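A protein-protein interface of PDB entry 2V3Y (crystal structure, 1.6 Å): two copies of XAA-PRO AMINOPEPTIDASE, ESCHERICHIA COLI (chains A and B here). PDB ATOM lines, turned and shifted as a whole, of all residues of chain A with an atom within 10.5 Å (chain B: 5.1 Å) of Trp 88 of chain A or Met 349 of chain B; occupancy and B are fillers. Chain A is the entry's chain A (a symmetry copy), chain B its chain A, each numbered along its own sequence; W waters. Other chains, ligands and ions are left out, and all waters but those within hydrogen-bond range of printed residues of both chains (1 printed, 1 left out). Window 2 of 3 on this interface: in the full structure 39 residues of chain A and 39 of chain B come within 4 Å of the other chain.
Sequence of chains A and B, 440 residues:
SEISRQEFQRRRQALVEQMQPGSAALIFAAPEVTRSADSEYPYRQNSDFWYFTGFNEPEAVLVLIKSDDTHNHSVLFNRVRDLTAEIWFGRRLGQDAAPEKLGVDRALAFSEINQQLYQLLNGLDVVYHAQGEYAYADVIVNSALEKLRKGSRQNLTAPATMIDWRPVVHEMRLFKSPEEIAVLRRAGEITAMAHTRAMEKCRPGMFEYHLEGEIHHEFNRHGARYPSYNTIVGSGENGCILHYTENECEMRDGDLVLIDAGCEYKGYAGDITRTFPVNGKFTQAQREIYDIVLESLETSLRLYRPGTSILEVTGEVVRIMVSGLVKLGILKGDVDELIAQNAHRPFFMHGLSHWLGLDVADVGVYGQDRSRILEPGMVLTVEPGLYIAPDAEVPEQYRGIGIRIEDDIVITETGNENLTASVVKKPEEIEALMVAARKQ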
ATOM      1  N   ARG A  79      -9.259  -2.524   6.719  1.00  0.00           N
ATOM      2  CA  ARG A  79      -9.652  -1.143   6.931  1.00  0.00           C
ATOM      3  C   ARG A  79     -10.365  -0.550   5.713  1.00  0.00           C
ATOM      4  O   ARG A  79      -9.946  -0.747   4.579  1.00  0.00           O
ATOM      5  CB  ARG A  79      -8.443  -0.290   7.271  1.00  0.00           C
ATOM      6  CG  ARG A  79      -7.882  -0.559   8.650  1.00  0.00           C
ATOM      7  CD  ARG A  79      -6.455  -0.041   8.783  1.00  0.00           C
ATOM      8  NE  ARG A  79      -6.167   0.410  10.141  1.00  0.00           N
ATOM      9  CZ  ARG A  79      -5.022   0.980  10.506  1.00  0.00           C
ATOM     10  NH1 ARG A  79      -4.066   1.204   9.617  1.00  0.00           N
ATOM     11  NH2 ARG A  79      -4.850   1.367  11.767  1.00  0.00           N
ATOM     12  N   ASP A  82     -10.836   5.733   3.530  1.00  0.00           N
ATOM     13  CA  ASP A  82     -11.179   6.879   4.376  1.00  0.00           C
ATOM     14  C   ASP A  82     -10.266   8.006   3.942  1.00  0.00           C
ATOM     15  O   ASP A  82      -9.068   7.967   4.209  1.00  0.00           O
ATOM     16  CB  ASP A  82     -10.961   6.531   5.860  1.00  0.00           C
ATOM     17  CG  ASP A  82     -11.364   7.644   6.819  1.00  0.00           C
ATOM     18  OD1 ASP A  82     -10.947   8.805   6.654  1.00  0.00           O
ATOM     19  OD2 ASP A  82     -12.096   7.339   7.783  1.00  0.00           O
ATOM     20  N   LEU A  83     -10.838   9.002   3.275  1.00  0.00           N
ATOM     21  CA  LEU A  83     -10.026  10.047   2.642  1.00  0.00           C
ATOM     22  C   LEU A  83      -9.124  10.758   3.660  1.00  0.00           C
ATOM     23  O   LEU A  83      -7.919  10.914   3.421  1.00  0.00           O
ATOM     24  CB  LEU A  83     -10.915  11.053   1.901  1.00  0.00           C
ATOM     25  CG  LEU A  83     -10.164  12.170   1.162  1.00  0.00           C
ATOM     26  CD1 LEU A  83      -9.167  11.586   0.145  1.00  0.00           C
ATOM     27  CD2 LEU A  83     -11.149  13.121   0.497  1.00  0.00           C
ATOM     28  N   THR A  84      -9.692  11.158   4.793  1.00  0.00           N
ATOM     29  CA  THR A  84      -8.922  11.883   5.816  1.00  0.00           C
ATOM     30  C   THR A  84      -7.829  11.026   6.456  1.00  0.00           C
ATOM     31  O   THR A  84      -6.691  11.476   6.610  1.00  0.00           O
ATOM     32  CB  THR A  84      -9.843  12.477   6.912  1.00  0.00           C
ATOM     33  OG1 THR A  84     -10.713  13.441   6.310  1.00  0.00           O
ATOM     34  CG2 THR A  84      -9.016  13.178   7.998  1.00  0.00           C
ATOM     35  N   ALA A  85      -8.157   9.785   6.802  1.00  0.00           N
ATOM     36  CA  ALA A  85      -7.172   8.894   7.402  1.00  0.00           C
ATOM     37  C   ALA A  85      -6.031   8.605   6.425  1.00  0.00           C
ATOM     38  O   ALA A  85      -4.866   8.503   6.824  1.00  0.00           O
ATOM     39  CB  ALA A  85      -7.838   7.583   7.860  1.00  0.00           C
ATOM     40  N   GLU A  86      -6.371   8.476   5.140  1.00  0.00           N
ATOM     41  CA  GLU A  86      -5.355   8.203   4.123  1.00  0.00           C
ATOM     42  C   GLU A  86      -4.466   9.424   3.829  1.00  0.00           C
ATOM     43  O   GLU A  86      -3.248   9.273   3.701  1.00  0.00           O
ATOM     44  CB  GLU A  86      -5.980   7.621   2.859  1.00  0.00           C
ATOM     45  CG  GLU A  86      -6.621   6.270   3.145  1.00  0.00           C
ATOM     46  CD  GLU A  86      -7.202   5.609   1.914  1.00  0.00           C
ATOM     47  OE1 GLU A  86      -6.461   5.429   0.917  1.00  0.00           O
ATOM     48  OE2 GLU A  86      -8.398   5.243   1.967  1.00  0.00           O
ATOM     49  N   ILE A  87      -5.051  10.619   3.745  1.00  0.00           N
ATOM     50  CA  ILE A  87      -4.249  11.852   3.618  1.00  0.00           C
ATOM     51  C   ILE A  87      -3.222  11.926   4.749  1.00  0.00           C
ATOM     52  O   ILE A  87      -2.075  12.323   4.552  1.00  0.00           O
ATOM     53  CB  ILE A  87      -5.134  13.125   3.668  1.00  0.00           C
ATOM     54  CG1 ILE A  87      -5.917  13.288   2.359  1.00  0.00           C
ATOM     55  CG2 ILE A  87      -4.298  14.390   3.968  1.00  0.00           C
ATOM     56  CD1 ILE A  87      -7.063  14.296   2.466  1.00  0.00           C
ATOM     57  N   TRP A  88      -3.650  11.577   5.951  1.00  0.00           N
ATOM     58  CA  TRP A  88      -2.768  11.667   7.105  1.00  0.00           C
ATOM     59  C   TRP A  88      -1.725  10.558   7.190  1.00  0.00           C
ATOM     60  O   TRP A  88      -0.544  10.831   7.446  1.00  0.00           O
ATOM     61  CB  TRP A  88      -3.598  11.741   8.399  1.00  0.00           C
ATOM     62  CG  TRP A  88      -4.043  13.136   8.648  1.00  0.00           C
ATOM     63  CD1 TRP A  88      -5.078  13.797   8.039  1.00  0.00           C
ATOM     64  CD2 TRP A  88      -3.426  14.094   9.525  1.00  0.00           C
ATOM     65  NE1 TRP A  88      -5.157  15.087   8.508  1.00  0.00           N
ATOM     66  CE2 TRP A  88      -4.155  15.293   9.415  1.00  0.00           C
ATOM     67  CE3 TRP A  88      -2.337  14.045  10.398  1.00  0.00           C
ATOM     68  CZ2 TRP A  88      -3.824  16.445  10.144  1.00  0.00           C
ATOM     69  CZ3 TRP A  88      -2.009  15.199  11.127  1.00  0.00           C
ATOM     70  CH2 TRP A  88      -2.757  16.369  10.994  1.00  0.00           C
ATOM     71  N   PHE A  89      -2.147   9.318   6.962  1.00  0.00           N
ATOM     72  CA  PHE A  89      -1.356   8.173   7.404  1.00  0.00           C
ATOM     73  C   PHE A  89      -0.983   7.156   6.329  1.00  0.00           C
ATOM     74  O   PHE A  89      -0.156   6.285   6.584  1.00  0.00           O
ATOM     75  CB  PHE A  89      -2.091   7.483   8.565  1.00  0.00           C
ATOM     76  CG  PHE A  89      -2.333   8.404   9.743  1.00  0.00           C
ATOM     77  CD1 PHE A  89      -1.264   9.006  10.395  1.00  0.00           C
ATOM     78  CD2 PHE A  89      -3.620   8.674  10.187  1.00  0.00           C
ATOM     79  CE1 PHE A  89      -1.473   9.861  11.469  1.00  0.00           C
ATOM     80  CE2 PHE A  89      -3.838   9.532  11.263  1.00  0.00           C
ATOM     81  CZ  PHE A  89      -2.765  10.121  11.905  1.00  0.00           C
ATOM     82  N   GLY A  90      -1.557   7.286   5.134  1.00  0.00           N
ATOM     83  CA  GLY A  90      -1.210   6.406   4.034  1.00  0.00           C
ATOM     84  C   GLY A  90      -2.398   5.738   3.395  1.00  0.00           C
ATOM     85  O   GLY A  90      -3.466   5.607   3.996  1.00  0.00           O
ATOM     86  N   ARG A  91      -2.181   5.262   2.175  1.00  0.00           N
ATOM     87  CA  ARG A  91      -3.241   4.651   1.408  1.00  0.00           C
ATOM     88  C   ARG A  91      -3.661   3.326   2.030  1.00  0.00           C
ATOM     89  O   ARG A  91      -2.855   2.646   2.678  1.00  0.00           O
ATOM     90  CB  ARG A  91      -2.810   4.445  -0.040  1.00  0.00           C
ATOM     91  CG  ARG A  91      -2.367   5.711  -0.749  1.00  0.00           C
ATOM     92  CD  ARG A  91      -2.173   5.475  -2.228  1.00  0.00           C
ATOM     93  NE  ARG A  91      -1.745   6.699  -2.891  1.00  0.00           N
ATOM     94  CZ  ARG A  91      -0.482   7.137  -2.935  1.00  0.00           C
ATOM     95  NH1 ARG A  91       0.507   6.444  -2.372  1.00  0.00           N
ATOM     96  NH2 ARG A  91      -0.216   8.255  -3.585  1.00  0.00           N
ATOM     97  N   ARG A  92      -4.935   2.997   1.845  1.00  0.00           N
ATOM     98  CA  ARG A  92      -5.524   1.743   2.282  1.00  0.00           C
ATOM     99  C   ARG A  92      -6.077   1.010   1.077  1.00  0.00           C
ATOM    100  O   ARG A  92      -6.590   1.627   0.114  1.00  0.00           O
ATOM    101  CB  ARG A  92      -6.677   2.014   3.232  1.00  0.00           C
ATOM    102  CG  ARG A  92      -6.263   2.603   4.546  1.00  0.00           C
ATOM    103  CD  ARG A  92      -7.465   3.110   5.268  1.00  0.00           C
ATOM    104  NE  ARG A  92      -7.113   3.593   6.598  1.00  0.00           N
ATOM    105  CZ  ARG A  92      -7.976   3.728   7.595  1.00  0.00           C
ATOM    106  NH1 ARG A  92      -9.258   3.446   7.424  1.00  0.00           N
ATOM    107  NH2 ARG A  92      -7.544   4.166   8.773  1.00  0.00           N
ATOM    108  N   ILE B 241       0.606  12.983   1.119  1.00  0.00           N
ATOM    109  CA  ILE B 241       0.259  12.148   2.264  1.00  0.00           C
ATOM    110  C   ILE B 241       1.195  12.504   3.420  1.00  0.00           C
ATOM    111  O   ILE B 241       2.423  12.367   3.311  1.00  0.00           O
ATOM    112  CB  ILE B 241       0.382  10.648   1.913  1.00  0.00           C
ATOM    113  CG1 ILE B 241      -0.614  10.287   0.808  1.00  0.00           C
ATOM    114  CG2 ILE B 241       0.124   9.779   3.174  1.00  0.00           C
ATOM    115  CD1 ILE B 241      -0.440   8.884   0.201  1.00  0.00           C
ATOM    116  N   LEU B 242       0.627  13.022   4.503  1.00  0.00           N
ATOM    117  CA  LEU B 242       1.426  13.671   5.533  1.00  0.00           C
ATOM    118  C   LEU B 242       2.502  12.793   6.205  1.00  0.00           C
ATOM    119  O   LEU B 242       3.627  13.258   6.482  1.00  0.00           O
ATOM    120  CB  LEU B 242       0.511  14.281   6.599  1.00  0.00           C
ATOM    121  CG  LEU B 242      -0.424  15.365   6.060  1.00  0.00           C
ATOM    122  CD1 LEU B 242      -1.253  15.947   7.223  1.00  0.00           C
ATOM    123  CD2 LEU B 242       0.314  16.499   5.316  1.00  0.00           C
ATOM    124  N   HIS B 243       2.117  11.560   6.516  1.00  0.00           N
ATOM    125  CA  HIS B 243       3.005  10.570   7.163  1.00  0.00           C
ATOM    126  C   HIS B 243       3.204   9.374   6.241  1.00  0.00           C
ATOM    127  O   HIS B 243       3.103   8.227   6.660  1.00  0.00           O
ATOM    128  CB  HIS B 243       2.432  10.130   8.516  1.00  0.00           C
ATOM    129  CG  HIS B 243       2.172  11.279   9.444  1.00  0.00           C
ATOM    130  ND1 HIS B 243       0.961  11.938   9.476  1.00  0.00           N
ATOM    131  CD2 HIS B 243       2.962  11.898  10.354  1.00  0.00           C
ATOM    132  CE1 HIS B 243       1.018  12.917  10.364  1.00  0.00           C
ATOM    133  NE2 HIS B 243       2.217  12.912  10.914  1.00  0.00           N
ATOM    134  N   TYR B 244       3.504   9.660   4.980  1.00  0.00           N
ATOM    135  CA  TYR B 244       3.780   8.609   4.002  1.00  0.00           C
ATOM    136  C   TYR B 244       5.090   7.904   4.365  1.00  0.00           C
ATOM    137  O   TYR B 244       6.154   8.512   4.280  1.00  0.00           O
ATOM    138  CB  TYR B 244       3.893   9.233   2.606  1.00  0.00           C
ATOM    139  CG  TYR B 244       4.330   8.247   1.545  1.00  0.00           C
ATOM    140  CD1 TYR B 244       3.426   7.381   0.945  1.00  0.00           C
ATOM    141  CD2 TYR B 244       5.658   8.212   1.124  1.00  0.00           C
ATOM    142  CE1 TYR B 244       3.830   6.484  -0.019  1.00  0.00           C
ATOM    143  CE2 TYR B 244       6.073   7.332   0.148  1.00  0.00           C
ATOM    144  CZ  TYR B 244       5.158   6.468  -0.435  1.00  0.00           C
ATOM    145  OH  TYR B 244       5.570   5.582  -1.412  1.00  0.00           O
ATOM    146  N   ARG B 345      -7.647  25.463   4.504  1.00  0.00           N
ATOM    147  CA  ARG B 345      -7.615  24.143   5.158  1.00  0.00           C
ATOM    148  C   ARG B 345      -7.551  22.919   4.233  1.00  0.00           C
ATOM    149  O   ARG B 345      -6.959  21.898   4.614  1.00  0.00           O
ATOM    150  CB  ARG B 345      -8.779  23.995   6.148  1.00  0.00           C
ATOM    151  CG  ARG B 345      -8.516  24.665   7.485  1.00  0.00           C
ATOM    152  CD  ARG B 345      -9.668  24.458   8.460  1.00  0.00           C
ATOM    153  NE  ARG B 345      -9.369  25.008   9.783  1.00  0.00           N
ATOM    154  CZ  ARG B 345     -10.268  25.201  10.747  1.00  0.00           C
ATOM    155  NH1 ARG B 345     -11.550  24.899  10.554  1.00  0.00           N
ATOM    156  NH2 ARG B 345      -9.881  25.705  11.913  1.00  0.00           N
ATOM    157  N   PRO B 346      -8.164  22.995   3.033  1.00  0.00           N
ATOM    158  CA  PRO B 346      -7.957  21.853   2.121  1.00  0.00           C
ATOM    159  C   PRO B 346      -6.496  21.641   1.712  1.00  0.00           C
ATOM    160  O   PRO B 346      -6.137  20.539   1.322  1.00  0.00           O
ATOM    161  CB  PRO B 346      -8.788  22.215   0.891  1.00  0.00           C
ATOM    162  CG  PRO B 346      -9.829  23.167   1.399  1.00  0.00           C
ATOM    163  CD  PRO B 346      -9.103  23.978   2.456  1.00  0.00           C
ATOM    164  N   PHE B 347      -5.679  22.693   1.820  1.00  0.00           N
ATOM    165  CA  PHE B 347      -4.285  22.668   1.360  1.00  0.00           C
ATOM    166  C   PHE B 347      -3.245  22.687   2.485  1.00  0.00           C
ATOM    167  O   PHE B 347      -2.115  22.225   2.290  1.00  0.00           O
ATOM    168  CB  PHE B 347      -4.041  23.837   0.399  1.00  0.00           C
ATOM    169  CG  PHE B 347      -5.073  23.933  -0.676  1.00  0.00           C
ATOM    170  CD1 PHE B 347      -5.146  22.938  -1.655  1.00  0.00           C
ATOM    171  CD2 PHE B 347      -6.016  24.948  -0.684  1.00  0.00           C
ATOM    172  CE1 PHE B 347      -6.125  22.981  -2.641  1.00  0.00           C
ATOM    173  CE2 PHE B 347      -6.991  25.008  -1.675  1.00  0.00           C
ATOM    174  CZ  PHE B 347      -7.049  24.016  -2.651  1.00  0.00           C
ATOM    175  N   PHE B 348      -3.622  23.236   3.647  1.00  0.00           N
ATOM    176  CA  PHE B 348      -2.779  23.227   4.848  1.00  0.00           C
ATOM    177  C   PHE B 348      -3.652  22.782   6.018  1.00  0.00           C
ATOM    178  O   PHE B 348      -4.364  23.593   6.621  1.00  0.00           O
ATOM    179  CB  PHE B 348      -2.165  24.598   5.101  1.00  0.00           C
ATOM    180  CG  PHE B 348      -1.380  24.704   6.376  1.00  0.00           C
ATOM    181  CD1 PHE B 348      -0.382  23.792   6.678  1.00  0.00           C
ATOM    182  CD2 PHE B 348      -1.586  25.777   7.266  1.00  0.00           C
ATOM    183  CE1 PHE B 348       0.369  23.909   7.824  1.00  0.00           C
ATOM    184  CE2 PHE B 348      -0.831  25.883   8.434  1.00  0.00           C
ATOM    185  CZ  PHE B 348       0.153  24.968   8.695  1.00  0.00           C
ATOM    186  N   MET B 349      -3.637  21.477   6.276  1.00  0.00           N
ATOM    187  CA  MET B 349      -4.625  20.854   7.165  1.00  0.00           C
ATOM    188  C   MET B 349      -4.062  20.394   8.500  1.00  0.00           C
ATOM    189  O   MET B 349      -4.763  19.704   9.271  1.00  0.00           O
ATOM    190  CB  MET B 349      -5.305  19.680   6.450  1.00  0.00           C
ATOM    191  CG  MET B 349      -4.427  18.453   6.170  1.00  0.00           C
ATOM    192  SD  MET B 349      -3.147  18.711   4.902  1.00  0.00           S
ATOM    193  CE  MET B 349      -4.113  19.071   3.435  1.00  0.00           C
ATOM    194  N   HIS B 350      -2.816  20.767   8.790  1.00  0.00           N
ATOM    195  CA  HIS B 350      -2.179  20.391  10.037  1.00  0.00           C
ATOM    196  C   HIS B 350      -1.655  21.632  10.761  1.00  0.00           C
ATOM    197  O   HIS B 350      -1.815  22.760  10.281  1.00  0.00           O
ATOM    198  CB  HIS B 350      -1.072  19.348   9.822  1.00  0.00           C
ATOM    199  CG  HIS B 350       0.046  19.803   8.936  1.00  0.00           C
ATOM    200  ND1 HIS B 350       1.076  20.607   9.394  1.00  0.00           N
ATOM    201  CD2 HIS B 350       0.331  19.519   7.641  1.00  0.00           C
ATOM    202  CE1 HIS B 350       1.925  20.826   8.398  1.00  0.00           C
ATOM    203  NE2 HIS B 350       1.503  20.169   7.327  1.00  0.00           N
ATOM    204  N   GLY B 351      -1.114  21.401  11.950  1.00  0.00           N
ATOM    205  CA  GLY B 351      -0.583  22.479  12.778  1.00  0.00           C
ATOM    206  C   GLY B 351       0.766  22.979  12.288  1.00  0.00           C
ATOM    207  O   GLY B 351       1.525  22.238  11.651  1.00  0.00           O
ATOM    208  N   TYR B 387      -0.397  21.163   0.274  1.00  0.00           N
ATOM    209  CA  TYR B 387      -0.602  19.869  -0.378  1.00  0.00           C
ATOM    210  C   TYR B 387      -1.781  20.015  -1.314  1.00  0.00           C
ATOM    211  O   TYR B 387      -2.901  20.250  -0.863  1.00  0.00           O
ATOM    212  CB  TYR B 387      -0.850  18.780   0.673  1.00  0.00           C
ATOM    213  CG  TYR B 387       0.100  18.927   1.850  1.00  0.00           C
ATOM    214  CD1 TYR B 387      -0.243  19.707   2.960  1.00  0.00           C
ATOM    215  CD2 TYR B 387       1.379  18.388   1.818  1.00  0.00           C
ATOM    216  CE1 TYR B 387       0.635  19.859   4.044  1.00  0.00           C
ATOM    217  CE2 TYR B 387       2.278  18.548   2.905  1.00  0.00           C
ATOM    218  CZ  TYR B 387       1.904  19.326   4.000  1.00  0.00           C
ATOM    219  OH  TYR B 387       2.749  19.497   5.059  1.00  0.00           O
HETATM  220  O   HOH W   1       2.322   5.349   5.246  1.00  0.00           O
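O of Ile 87 of chain A lies within hydrogen-bond range of N of Leu 242 of chain B (2.8 Å).
ND1 of His 243 of chain B is in hydrogen-bond range of O of Trp 88 of chain A (2.8 Å).
The side-chain carboxylate (OE2) of Glu 86 of chain A lies within hydrogen-bond range of the backbone NH (N) of Asp 82 of chain A (2.9 Å).
The side-chain carboxylate (OE1) of Glu 86 of chain A sits at hydrogen-bond distance from the backbone NH (N) of Arg 92 of chain A.
The side-chain hydroxyl of Tyr 387 of chain B is in hydrogen-bond range of a ring nitrogen (NE2) of His 350 of chain B (2.7 Å).
Among the printed residues, pairs that only touch across the chains: Glu 86 of chain A with Ile 241 of chain B (3.5 Å), Ile 87 of chain A with Ile 241 of chain B (3.3 Å), Trp 88 of chain A with Leu 242 of chain B (3.7 Å), Trp 88 of chain A with Met 349 of chain B (3.5 Å), Trp 88 of chain A with His 350 of chain B (3.6 Å), Phe 89 of chain A with His 243 of chain B (3.8 Å), Gly 90 of chain A with Ile 241 of chain B (3.6 Å) and Arg 91 of chain A with Ile 241 of chain B (3.6 Å).
Of chain B, only Leu 242 (3.7 Å), His 243 (2.8 Å), Met 349 (3.5 Å) and His 350 (3.6 Å) come within 4 Å of Trp 88 of chain A.
Printed residues of chain A within 4 Å of Leu 242 of chain B: Ile 87 (2.8 Å) and Trp 88 (3.7 Å).
Of chain A, only Trp 88 and Phe 89 come within 4 Å of His 243 of chain B.
No residue of chain A comes within 4 Å of Phe 348 of chain B.
Of chain A, only Trp 88 comes within 4 Å of His 350 of chain B.
Printed residues of chain A within 4 Å of Ile 241 of chain B: Glu 86 (3.5 Å), Ile 87 (3.3 Å), Gly 90 (3.6 Å) and Arg 91 (3.6 Å).
Printed residues of chain B within 4 Å of Glu 86 of chain A: Ile 241 (3.5 Å).
Leu 83 of chain A touches none of the printed residues of chain B.
Phe 347 of chain B touches none of the printed residues of chain A.
The nearest residue of chain A that does not touch Met 349 of chain B is Ile 87 of chain A (4.6 Å).
Of the 12 printed residues of chain B, 5 touch a printed residue of chain A.
Hydrophobic or aromatic side chains of chain B that line the printed part of chain A: Ile 241, Leu 242, His 243 and His 350.
Printed residues of chain A that touch a printed residue of chain B: Glu 86, Ile 87, Trp 88, Phe 89, Gly 90 and Arg 91.
Hydrophobic or aromatic side chains of chain A that line the printed part of chain B: Trp 88 and Phe 89.
Among the printed residues, 10 pairs touch across the chains.
No position is printed for both chains.
Water W1 bridges O of Phe 89 of chain A (3.0 Å) and O of His 243 of chain B (3.3 Å).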
